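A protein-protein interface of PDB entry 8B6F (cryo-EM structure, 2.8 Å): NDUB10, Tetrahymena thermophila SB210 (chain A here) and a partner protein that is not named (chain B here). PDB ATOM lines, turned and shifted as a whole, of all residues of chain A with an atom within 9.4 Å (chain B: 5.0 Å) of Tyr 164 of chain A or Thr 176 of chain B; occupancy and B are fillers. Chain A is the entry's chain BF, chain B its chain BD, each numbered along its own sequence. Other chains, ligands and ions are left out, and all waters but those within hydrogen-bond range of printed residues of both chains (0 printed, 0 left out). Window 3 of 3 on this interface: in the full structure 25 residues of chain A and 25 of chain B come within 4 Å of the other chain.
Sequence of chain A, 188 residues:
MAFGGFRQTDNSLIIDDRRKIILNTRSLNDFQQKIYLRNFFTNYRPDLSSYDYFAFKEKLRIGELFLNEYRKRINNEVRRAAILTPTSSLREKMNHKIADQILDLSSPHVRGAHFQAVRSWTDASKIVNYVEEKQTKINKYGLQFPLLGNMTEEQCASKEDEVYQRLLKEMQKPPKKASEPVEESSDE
The backbone carbonyl oxygen (O) of Arg 172 of chain B lies close to the side-chain hydroxyl (OG1) of Thr 176 of chain B, 3.3 Å away.
The backbone carbonyl oxygen (O) of Ala 173 of chain B sits at hydrogen-bond distance from the side-chain hydroxyl (OG1) of Thr 176 of chain B, at 2.7 Å.
Lys 159 of chain A touches none of the printed residues of chain B.
Of the printed residues of chain B, Glu 160 of chain A touches Ala 169 (3.8 Å) and Arg 172 (3.8 Å).
Tyr 164 of chain A touches four residues of chain B.
Printed residues of chain B within 4 Å of Met 171 of chain A: Ala 173 and Asn 177.
Of the printed residues of chain B, Gln 172 of chain A touches Tyr 180 (3.7 Å).
Of chain A, only Tyr 164, Leu 167, Leu 168 and Met 171 come within 4 Å of Ala 173 of chain B.
Of chain A, only Tyr 164 and Leu 168 come within 4 Å of Thr 176 of chain B.
Of the printed residues of chain A, Asn 177 of chain B touches Met 171.
No residue of chain A comes within 4 Å of Glu 179 of chain B.
Of the printed residues of chain A, Tyr 180 of chain B touches Gln 172.
The nearest residue of chain A that does not touch Thr 176 of chain B is Met 171 of chain A (5.4 Å).
OE2 of Glu 160 of chain A lies within salt-bridge range of NH1 of Arg 172 of chain B (3.9 Å).
Among the printed residues, merely in contact across the chains: Tyr 164 of chain A with Thr 176 of chain B, Leu 168 of chain A with Thr 176 of chain B, Tyr 164 of chain A with Arg 172 of chain B, Val 163 of chain A with Ala 169 of chain B, Gln 172 of chain A with Tyr 180 of chain B, Met 171 of chain A with Ala 173 of chain B, Leu 168 of chain A with Ala 173 of chain B, Leu 167 of chain A with Ala 173 of chain B, Glu 160 of chain A with Ala 169 of chain B, Tyr 164 of chain A with Ala 169 of chain B, Tyr 164 of chain A with Ala 173 of chain B, Leu 167 of chain A with Ala 169 of chain B and Met 171 of chain A with Asn 177 of chain B.
Of the 20 printed residues of chain A, 7 touch a printed residue of chain B.
Printed residues of chain B that touch a printed residue of chain A: Ala 169, Arg 172, Ala 173, Thr 176, Asn 177 and Tyr 180.
Hydrophobic or aromatic side chains of chain B within 4 Å of the printed part of chain A: Ala 169, Ala 173 and Tyr 180.
Among the printed residues, 14 pairs touch across the chains.
Among the printed residues, Asp or Glu carboxylates within 4 Å of a Lys or Arg side-chain nitrogen of the other chain: Glu 160 of chain A with Arg 172 of chain B.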
ATOM      1  N   LYS A 140      19.739 -13.271  31.589  1.00  0.00           N
ATOM      2  CA  LYS A 140      18.924 -12.141  31.153  1.00  0.00           C
ATOM      3  C   LYS A 140      19.742 -11.179  30.303  1.00  0.00           C
ATOM      4  O   LYS A 140      19.282 -10.716  29.253  1.00  0.00           O
ATOM      5  CB  LYS A 140      18.339 -11.403  32.359  1.00  0.00           C
ATOM      6  CG  LYS A 140      17.203 -12.130  33.051  1.00  0.00           C
ATOM      7  CD  LYS A 140      16.406 -11.201  33.956  1.00  0.00           C
ATOM      8  CE  LYS A 140      17.293 -10.464  34.950  1.00  0.00           C
ATOM      9  NZ  LYS A 140      16.492  -9.669  35.923  1.00  0.00           N
ATOM     10  N   TYR A 141      20.957 -10.867  30.745  1.00  0.00           N
ATOM     11  CA  TYR A 141      21.849  -9.967  30.030  1.00  0.00           C
ATOM     12  C   TYR A 141      22.920 -10.700  29.236  1.00  0.00           C
ATOM     13  O   TYR A 141      23.754 -10.051  28.600  1.00  0.00           O
ATOM     14  CB  TYR A 141      22.504  -8.999  31.017  1.00  0.00           C
ATOM     15  CG  TYR A 141      21.512  -8.368  31.964  1.00  0.00           C
ATOM     16  CD1 TYR A 141      20.642  -7.378  31.529  1.00  0.00           C
ATOM     17  CD2 TYR A 141      21.440  -8.766  33.293  1.00  0.00           C
ATOM     18  CE1 TYR A 141      19.728  -6.801  32.389  1.00  0.00           C
ATOM     19  CE2 TYR A 141      20.530  -8.196  34.161  1.00  0.00           C
ATOM     20  CZ  TYR A 141      19.677  -7.214  33.704  1.00  0.00           C
ATOM     21  OH  TYR A 141      18.770  -6.641  34.563  1.00  0.00           O
ATOM     22  N   GLY A 142      22.924 -12.028  29.260  1.00  0.00           N
ATOM     23  CA  GLY A 142      23.844 -12.788  28.434  1.00  0.00           C
ATOM     24  C   GLY A 142      25.298 -12.600  28.804  1.00  0.00           C
ATOM     25  O   GLY A 142      26.141 -12.425  27.918  1.00  0.00           O
ATOM     26  N   CYS A 156      25.290 -15.911  19.341  1.00  0.00           N
ATOM     27  CA  CYS A 156      25.813 -14.720  20.002  1.00  0.00           C
ATOM     28  C   CYS A 156      25.156 -13.458  19.460  1.00  0.00           C
ATOM     29  O   CYS A 156      24.796 -12.558  20.228  1.00  0.00           O
ATOM     30  CB  CYS A 156      27.329 -14.647  19.832  1.00  0.00           C
ATOM     31  SG  CYS A 156      28.232 -15.995  20.617  1.00  0.00           S
ATOM     32  N   ALA A 157      24.989 -13.372  18.141  1.00  0.00           N
ATOM     33  CA  ALA A 157      24.359 -12.193  17.559  1.00  0.00           C
ATOM     34  C   ALA A 157      22.909 -12.067  18.008  1.00  0.00           C
ATOM     35  O   ALA A 157      22.456 -10.975  18.369  1.00  0.00           O
ATOM     36  CB  ALA A 157      24.449 -12.246  16.035  1.00  0.00           C
ATOM     37  N   SER A 158      22.164 -13.173  17.994  1.00  0.00           N
ATOM     38  CA  SER A 158      20.775 -13.128  18.439  1.00  0.00           C
ATOM     39  C   SER A 158      20.685 -12.729  19.905  1.00  0.00           C
ATOM     40  O   SER A 158      19.807 -11.950  20.293  1.00  0.00           O
ATOM     41  CB  SER A 158      20.105 -14.483  18.215  1.00  0.00           C
ATOM     42  OG  SER A 158      20.108 -14.833  16.843  1.00  0.00           O
ATOM     43  N   LYS A 159      21.580 -13.262  20.737  1.00  0.00           N
ATOM     44  CA  LYS A 159      21.580 -12.904  22.151  1.00  0.00           C
ATOM     45  C   LYS A 159      21.919 -11.433  22.350  1.00  0.00           C
ATOM     46  O   LYS A 159      21.322 -10.766  23.202  1.00  0.00           O
ATOM     47  CB  LYS A 159      22.565 -13.790  22.915  1.00  0.00           C
ATOM     48  CG  LYS A 159      22.477 -13.667  24.433  1.00  0.00           C
ATOM     49  CD  LYS A 159      21.145 -14.178  24.960  1.00  0.00           C
ATOM     50  CE  LYS A 159      21.088 -14.124  26.477  1.00  0.00           C
ATOM     51  NZ  LYS A 159      19.777 -14.606  26.995  1.00  0.00           N
ATOM     52  N   GLU A 160      22.857 -10.898  21.565  1.00  0.00           N
ATOM     53  CA  GLU A 160      23.177  -9.478  21.670  1.00  0.00           C
ATOM     54  C   GLU A 160      21.963  -8.622  21.338  1.00  0.00           C
ATOM     55  O   GLU A 160      21.664  -7.652  22.041  1.00  0.00           O
ATOM     56  CB  GLU A 160      24.342  -9.126  20.745  1.00  0.00           C
ATOM     57  CG  GLU A 160      24.813  -7.680  20.878  1.00  0.00           C
ATOM     58  CD  GLU A 160      25.733  -7.254  19.749  1.00  0.00           C
ATOM     59  OE1 GLU A 160      25.977  -8.069  18.838  1.00  0.00           O
ATOM     60  OE2 GLU A 160      26.206  -6.100  19.768  1.00  0.00           O
ATOM     61  N   ASP A 161      21.250  -8.964  20.265  1.00  0.00           N
ATOM     62  CA  ASP A 161      20.057  -8.203  19.912  1.00  0.00           C
ATOM     63  C   ASP A 161      19.008  -8.302  21.010  1.00  0.00           C
ATOM     64  O   ASP A 161      18.376  -7.302  21.371  1.00  0.00           O
ATOM     65  CB  ASP A 161      19.492  -8.699  18.582  1.00  0.00           C
ATOM     66  CG  ASP A 161      18.275  -7.913  18.139  1.00  0.00           C
ATOM     67  OD1 ASP A 161      18.425  -6.713  17.825  1.00  0.00           O
ATOM     68  OD2 ASP A 161      17.170  -8.492  18.104  1.00  0.00           O
ATOM     69  N   GLU A 162      18.808  -9.504  21.552  1.00  0.00           N
ATOM     70  CA  GLU A 162      17.831  -9.686  22.620  1.00  0.00           C
ATOM     71  C   GLU A 162      18.198  -8.863  23.848  1.00  0.00           C
ATOM     72  O   GLU A 162      17.335  -8.216  24.452  1.00  0.00           O
ATOM     73  CB  GLU A 162      17.730 -11.169  22.976  1.00  0.00           C
ATOM     74  CG  GLU A 162      16.789 -11.474  24.128  1.00  0.00           C
ATOM     75  CD  GLU A 162      16.750 -12.950  24.462  1.00  0.00           C
ATOM     76  OE1 GLU A 162      17.374 -13.742  23.725  1.00  0.00           O
ATOM     77  OE2 GLU A 162      16.100 -13.319  25.462  1.00  0.00           O
ATOM     78  N   VAL A 163      19.475  -8.876  24.234  1.00  0.00           N
ATOM     79  CA  VAL A 163      19.906  -8.130  25.412  1.00  0.00           C
ATOM     80  C   VAL A 163      19.772  -6.633  25.170  1.00  0.00           C
ATOM     81  O   VAL A 163      19.405  -5.874  26.073  1.00  0.00           O
ATOM     82  CB  VAL A 163      21.346  -8.521  25.791  1.00  0.00           C
ATOM     83  CG1 VAL A 163      21.874  -7.633  26.910  1.00  0.00           C
ATOM     84  CG2 VAL A 163      21.395  -9.977  26.215  1.00  0.00           C
ATOM     85  N   TYR A 164      20.059  -6.185  23.949  1.00  0.00           N
ATOM     86  CA  TYR A 164      19.882  -4.777  23.617  1.00  0.00           C
ATOM     87  C   TYR A 164      18.425  -4.360  23.774  1.00  0.00           C
ATOM     88  O   TYR A 164      18.125  -3.325  24.375  1.00  0.00           O
ATOM     89  CB  TYR A 164      20.378  -4.527  22.193  1.00  0.00           C
ATOM     90  CG  TYR A 164      20.006  -3.185  21.617  1.00  0.00           C
ATOM     91  CD1 TYR A 164      20.738  -2.041  21.913  1.00  0.00           C
ATOM     92  CD2 TYR A 164      18.929  -3.069  20.751  1.00  0.00           C
ATOM     93  CE1 TYR A 164      20.394  -0.817  21.367  1.00  0.00           C
ATOM     94  CE2 TYR A 164      18.579  -1.858  20.205  1.00  0.00           C
ATOM     95  CZ  TYR A 164      19.310  -0.737  20.514  1.00  0.00           C
ATOM     96  OH  TYR A 164      18.939   0.457  19.953  1.00  0.00           O
ATOM     97  N   GLN A 165      17.501  -5.163  23.245  1.00  0.00           N
ATOM     98  CA  GLN A 165      16.085  -4.845  23.392  1.00  0.00           C
ATOM     99  C   GLN A 165      15.676  -4.831  24.860  1.00  0.00           C
ATOM    100  O   GLN A 165      14.943  -3.939  25.301  1.00  0.00           O
ATOM    101  CB  GLN A 165      15.236  -5.846  22.608  1.00  0.00           C
ATOM    102  CG  GLN A 165      15.418  -5.769  21.102  1.00  0.00           C
ATOM    103  CD  GLN A 165      14.937  -4.456  20.522  1.00  0.00           C
ATOM    104  OE1 GLN A 165      14.325  -3.645  21.214  1.00  0.00           O
ATOM    105  NE2 GLN A 165      15.213  -4.239  19.241  1.00  0.00           N
ATOM    106  N   ARG A 166      16.138  -5.817  25.630  1.00  0.00           N
ATOM    107  CA  ARG A 166      15.784  -5.886  27.043  1.00  0.00           C
ATOM    108  C   ARG A 166      16.303  -4.672  27.802  1.00  0.00           C
ATOM    109  O   ARG A 166      15.581  -4.083  28.613  1.00  0.00           O
ATOM    110  CB  ARG A 166      16.333  -7.174  27.656  1.00  0.00           C
ATOM    111  CG  ARG A 166      16.069  -7.315  29.147  1.00  0.00           C
ATOM    112  CD  ARG A 166      16.643  -8.610  29.682  1.00  0.00           C
ATOM    113  NE  ARG A 166      15.992  -9.780  29.102  1.00  0.00           N
ATOM    114  CZ  ARG A 166      14.922 -10.379  29.607  1.00  0.00           C
ATOM    115  NH1 ARG A 166      14.339  -9.941  30.711  1.00  0.00           N
ATOM    116  NH2 ARG A 166      14.427 -11.447  28.990  1.00  0.00           N
ATOM    117  N   LEU A 167      17.552  -4.277  27.547  1.00  0.00           N
ATOM    118  CA  LEU A 167      18.109  -3.110  28.222  1.00  0.00           C
ATOM    119  C   LEU A 167      17.351  -1.845  27.850  1.00  0.00           C
ATOM    120  O   LEU A 167      17.095  -0.992  28.708  1.00  0.00           O
ATOM    121  CB  LEU A 167      19.591  -2.966  27.882  1.00  0.00           C
ATOM    122  CG  LEU A 167      20.528  -4.029  28.463  1.00  0.00           C
ATOM    123  CD1 LEU A 167      21.938  -3.807  27.958  1.00  0.00           C
ATOM    124  CD2 LEU A 167      20.498  -4.022  29.985  1.00  0.00           C
ATOM    125  N   LEU A 168      16.987  -1.698  26.576  1.00  0.00           N
ATOM    126  CA  LEU A 168      16.211  -0.533  26.168  1.00  0.00           C
ATOM    127  C   LEU A 168      14.880  -0.480  26.904  1.00  0.00           C
ATOM    128  O   LEU A 168      14.485   0.569  27.423  1.00  0.00           O
ATOM    129  CB  LEU A 168      15.986  -0.557  24.655  1.00  0.00           C
ATOM    130  CG  LEU A 168      16.939   0.276  23.800  1.00  0.00           C
ATOM    131  CD1 LEU A 168      16.766   1.756  24.109  1.00  0.00           C
ATOM    132  CD2 LEU A 168      18.375  -0.165  24.030  1.00  0.00           C
ATOM    133  N   LYS A 169      14.176  -1.611  26.970  1.00  0.00           N
ATOM    134  CA  LYS A 169      12.888  -1.636  27.654  1.00  0.00           C
ATOM    135  C   LYS A 169      13.045  -1.326  29.137  1.00  0.00           C
ATOM    136  O   LYS A 169      12.250  -0.570  29.708  1.00  0.00           O
ATOM    137  CB  LYS A 169      12.217  -2.994  27.453  1.00  0.00           C
ATOM    138  CG  LYS A 169      10.827  -3.086  28.059  1.00  0.00           C
ATOM    139  CD  LYS A 169      10.072  -4.304  27.551  1.00  0.00           C
ATOM    140  CE  LYS A 169      10.777  -5.601  27.923  1.00  0.00           C
ATOM    141  NZ  LYS A 169      10.011  -6.796  27.471  1.00  0.00           N
ATOM    142  N   GLU A 170      14.067  -1.897  29.778  1.00  0.00           N
ATOM    143  CA  GLU A 170      14.285  -1.642  31.198  1.00  0.00           C
ATOM    144  C   GLU A 170      14.579  -0.171  31.459  1.00  0.00           C
ATOM    145  O   GLU A 170      14.065   0.413  32.419  1.00  0.00           O
ATOM    146  CB  GLU A 170      15.429  -2.514  31.716  1.00  0.00           C
ATOM    147  CG  GLU A 170      15.122  -4.000  31.724  1.00  0.00           C
ATOM    148  CD  GLU A 170      14.031  -4.365  32.707  1.00  0.00           C
ATOM    149  OE1 GLU A 170      13.617  -3.485  33.490  1.00  0.00           O
ATOM    150  OE2 GLU A 170      13.588  -5.531  32.698  1.00  0.00           O
ATOM    151  N   MET A 171      15.409   0.445  30.616  1.00  0.00           N
ATOM    152  CA  MET A 171      15.702   1.866  30.770  1.00  0.00           C
ATOM    153  C   MET A 171      14.450   2.714  30.582  1.00  0.00           C
ATOM    154  O   MET A 171      14.212   3.662  31.338  1.00  0.00           O
ATOM    155  CB  MET A 171      16.787   2.285  29.778  1.00  0.00           C
ATOM    156  CG  MET A 171      18.151   1.669  30.059  1.00  0.00           C
ATOM    157  SD  MET A 171      19.363   2.041  28.778  1.00  0.00           S
ATOM    158  CE  MET A 171      20.788   1.150  29.392  1.00  0.00           C
ATOM    159  N   GLN A 172      13.633   2.386  29.579  1.00  0.00           N
ATOM    160  CA  GLN A 172      12.418   3.153  29.330  1.00  0.00           C
ATOM    161  C   GLN A 172      11.390   2.993  30.446  1.00  0.00           C
ATOM    162  O   GLN A 172      10.550   3.879  30.636  1.00  0.00           O
ATOM    163  CB  GLN A 172      11.803   2.739  27.991  1.00  0.00           C
ATOM    164  CG  GLN A 172      12.666   3.065  26.777  1.00  0.00           C
ATOM    165  CD  GLN A 172      12.982   4.545  26.656  1.00  0.00           C
ATOM    166  OE1 GLN A 172      14.123   4.925  26.396  1.00  0.00           O
ATOM    167  NE2 GLN A 172      11.969   5.386  26.838  1.00  0.00           N
ATOM    168  N   ALA B 169      26.015  -4.993  23.867  1.00  0.00           N
ATOM    169  CA  ALA B 169      24.614  -4.636  24.063  1.00  0.00           C
ATOM    170  C   ALA B 169      24.478  -3.437  24.993  1.00  0.00           C
ATOM    171  O   ALA B 169      23.666  -2.538  24.748  1.00  0.00           O
ATOM    172  CB  ALA B 169      23.840  -5.831  24.617  1.00  0.00           C
ATOM    173  N   ARG B 172      25.510  -0.215  23.160  1.00  0.00           N
ATOM    174  CA  ARG B 172      24.444   0.243  22.276  1.00  0.00           C
ATOM    175  C   ARG B 172      23.294   0.845  23.071  1.00  0.00           C
ATOM    176  O   ARG B 172      22.755   1.893  22.699  1.00  0.00           O
ATOM    177  CB  ARG B 172      23.944  -0.912  21.411  1.00  0.00           C
ATOM    178  CG  ARG B 172      24.970  -1.445  20.430  1.00  0.00           C
ATOM    179  CD  ARG B 172      24.457  -2.698  19.744  1.00  0.00           C
ATOM    180  NE  ARG B 172      23.205  -2.454  19.040  1.00  0.00           N
ATOM    181  CZ  ARG B 172      22.412  -3.405  18.566  1.00  0.00           C
ATOM    182  NH1 ARG B 172      22.703  -4.686  18.717  1.00  0.00           N
ATOM    183  NH2 ARG B 172      21.299  -3.061  17.926  1.00  0.00           N
ATOM    184  N   ALA B 173      22.912   0.202  24.175  1.00  0.00           N
ATOM    185  CA  ALA B 173      21.814   0.714  24.987  1.00  0.00           C
ATOM    186  C   ALA B 173      22.155   2.073  25.582  1.00  0.00           C
ATOM    187  O   ALA B 173      21.307   2.971  25.623  1.00  0.00           O
ATOM    188  CB  ALA B 173      21.469  -0.284  26.092  1.00  0.00           C
ATOM    189  N   LEU B 174      23.389   2.243  26.057  1.00  0.00           N
ATOM    190  CA  LEU B 174      23.799   3.539  26.586  1.00  0.00           C
ATOM    191  C   LEU B 174      23.769   4.616  25.509  1.00  0.00           C
ATOM    192  O   LEU B 174      23.328   5.742  25.762  1.00  0.00           O
ATOM    193  CB  LEU B 174      25.193   3.449  27.202  1.00  0.00           C
ATOM    194  CG  LEU B 174      25.331   2.738  28.551  1.00  0.00           C
ATOM    195  CD1 LEU B 174      26.782   2.754  28.982  1.00  0.00           C
ATOM    196  CD2 LEU B 174      24.451   3.371  29.618  1.00  0.00           C
ATOM    197  N   ALA B 175      24.231   4.292  24.300  1.00  0.00           N
ATOM    198  CA  ALA B 175      24.193   5.271  23.219  1.00  0.00           C
ATOM    199  C   ALA B 175      22.761   5.688  22.909  1.00  0.00           C
ATOM    200  O   ALA B 175      22.467   6.879  22.760  1.00  0.00           O
ATOM    201  CB  ALA B 175      24.866   4.694  21.974  1.00  0.00           C
ATOM    202  N   THR B 176      21.851   4.720  22.817  1.00  0.00           N
ATOM    203  CA  THR B 176      20.459   5.037  22.516  1.00  0.00           C
ATOM    204  C   THR B 176      19.832   5.860  23.631  1.00  0.00           C
ATOM    205  O   THR B 176      19.075   6.802  23.369  1.00  0.00           O
ATOM    206  CB  THR B 176      19.666   3.755  22.293  1.00  0.00           C
ATOM    207  OG1 THR B 176      19.713   2.957  23.480  1.00  0.00           O
ATOM    208  CG2 THR B 176      20.231   2.982  21.129  1.00  0.00           C
ATOM    209  N   ASN B 177      20.132   5.516  24.883  1.00  0.00           N
ATOM    210  CA  ASN B 177      19.607   6.286  26.002  1.00  0.00           C
ATOM    211  C   ASN B 177      20.134   7.713  25.972  1.00  0.00           C
ATOM    212  O   ASN B 177      19.391   8.662  26.247  1.00  0.00           O
ATOM    213  CB  ASN B 177      19.977   5.608  27.320  1.00  0.00           C
ATOM    214  CG  ASN B 177      19.591   6.435  28.527  1.00  0.00           C
ATOM    215  OD1 ASN B 177      20.330   6.500  29.509  1.00  0.00           O
ATOM    216  ND2 ASN B 177      18.422   7.063  28.470  1.00  0.00           N
ATOM    217  N   GLN B 178      21.414   7.886  25.639  1.00  0.00           N
ATOM    218  CA  GLN B 178      21.969   9.231  25.548  1.00  0.00           C
ATOM    219  C   GLN B 178      21.277  10.030  24.453  1.00  0.00           C
ATOM    220  O   GLN B 178      20.971  11.213  24.636  1.00  0.00           O
ATOM    221  CB  GLN B 178      23.474   9.156  25.292  1.00  0.00           C
ATOM    222  CG  GLN B 178      24.192  10.490  25.408  1.00  0.00           C
ATOM    223  CD  GLN B 178      24.180  11.038  26.818  1.00  0.00           C
ATOM    224  OE1 GLN B 178      23.755  10.365  27.756  1.00  0.00           O
ATOM    225  NE2 GLN B 178      24.646  12.272  26.977  1.00  0.00           N
ATOM    226  N   GLU B 179      21.027   9.404  23.300  1.00  0.00           N
ATOM    227  CA  GLU B 179      20.304  10.092  22.236  1.00  0.00           C
ATOM    228  C   GLU B 179      18.897  10.460  22.685  1.00  0.00           C
ATOM    229  O   GLU B 179      18.410  11.558  22.396  1.00  0.00           O
ATOM    230  CB  GLU B 179      20.253   9.226  20.976  1.00  0.00           C
ATOM    231  CG  GLU B 179      21.449   9.398  20.046  1.00  0.00           C
ATOM    232  CD  GLU B 179      22.526   8.353  20.267  1.00  0.00           C
ATOM    233  OE1 GLU B 179      22.197   7.149  20.256  1.00  0.00           O
ATOM    234  OE2 GLU B 179      23.702   8.734  20.449  1.00  0.00           O
ATOM    235  N   TYR B 180      18.227   9.547  23.392  1.00  0.00           N
ATOM    236  CA  TYR B 180      16.884   9.826  23.887  1.00  0.00           C
ATOM    237  C   TYR B 180      16.886  11.003  24.854  1.00  0.00           C
ATOM    238  O   TYR B 180      16.020  11.881  24.778  1.00  0.00           O
ATOM    239  CB  TYR B 180      16.320   8.573  24.557  1.00  0.00           C
ATOM    240  CG  TYR B 180      14.937   8.730  25.143  1.00  0.00           C
ATOM    241  CD1 TYR B 180      13.809   8.688  24.333  1.00  0.00           C
ATOM    242  CD2 TYR B 180      14.757   8.879  26.511  1.00  0.00           C
ATOM    243  CE1 TYR B 180      12.541   8.813  24.866  1.00  0.00           C
ATOM    244  CE2 TYR B 180      13.493   9.005  27.056  1.00  0.00           C
ATOM    245  CZ  TYR B 180      12.390   8.970  26.228  1.00  0.00           C
ATOM    246  OH  TYR B 180      11.131   9.098  26.768  1.00  0.00           O
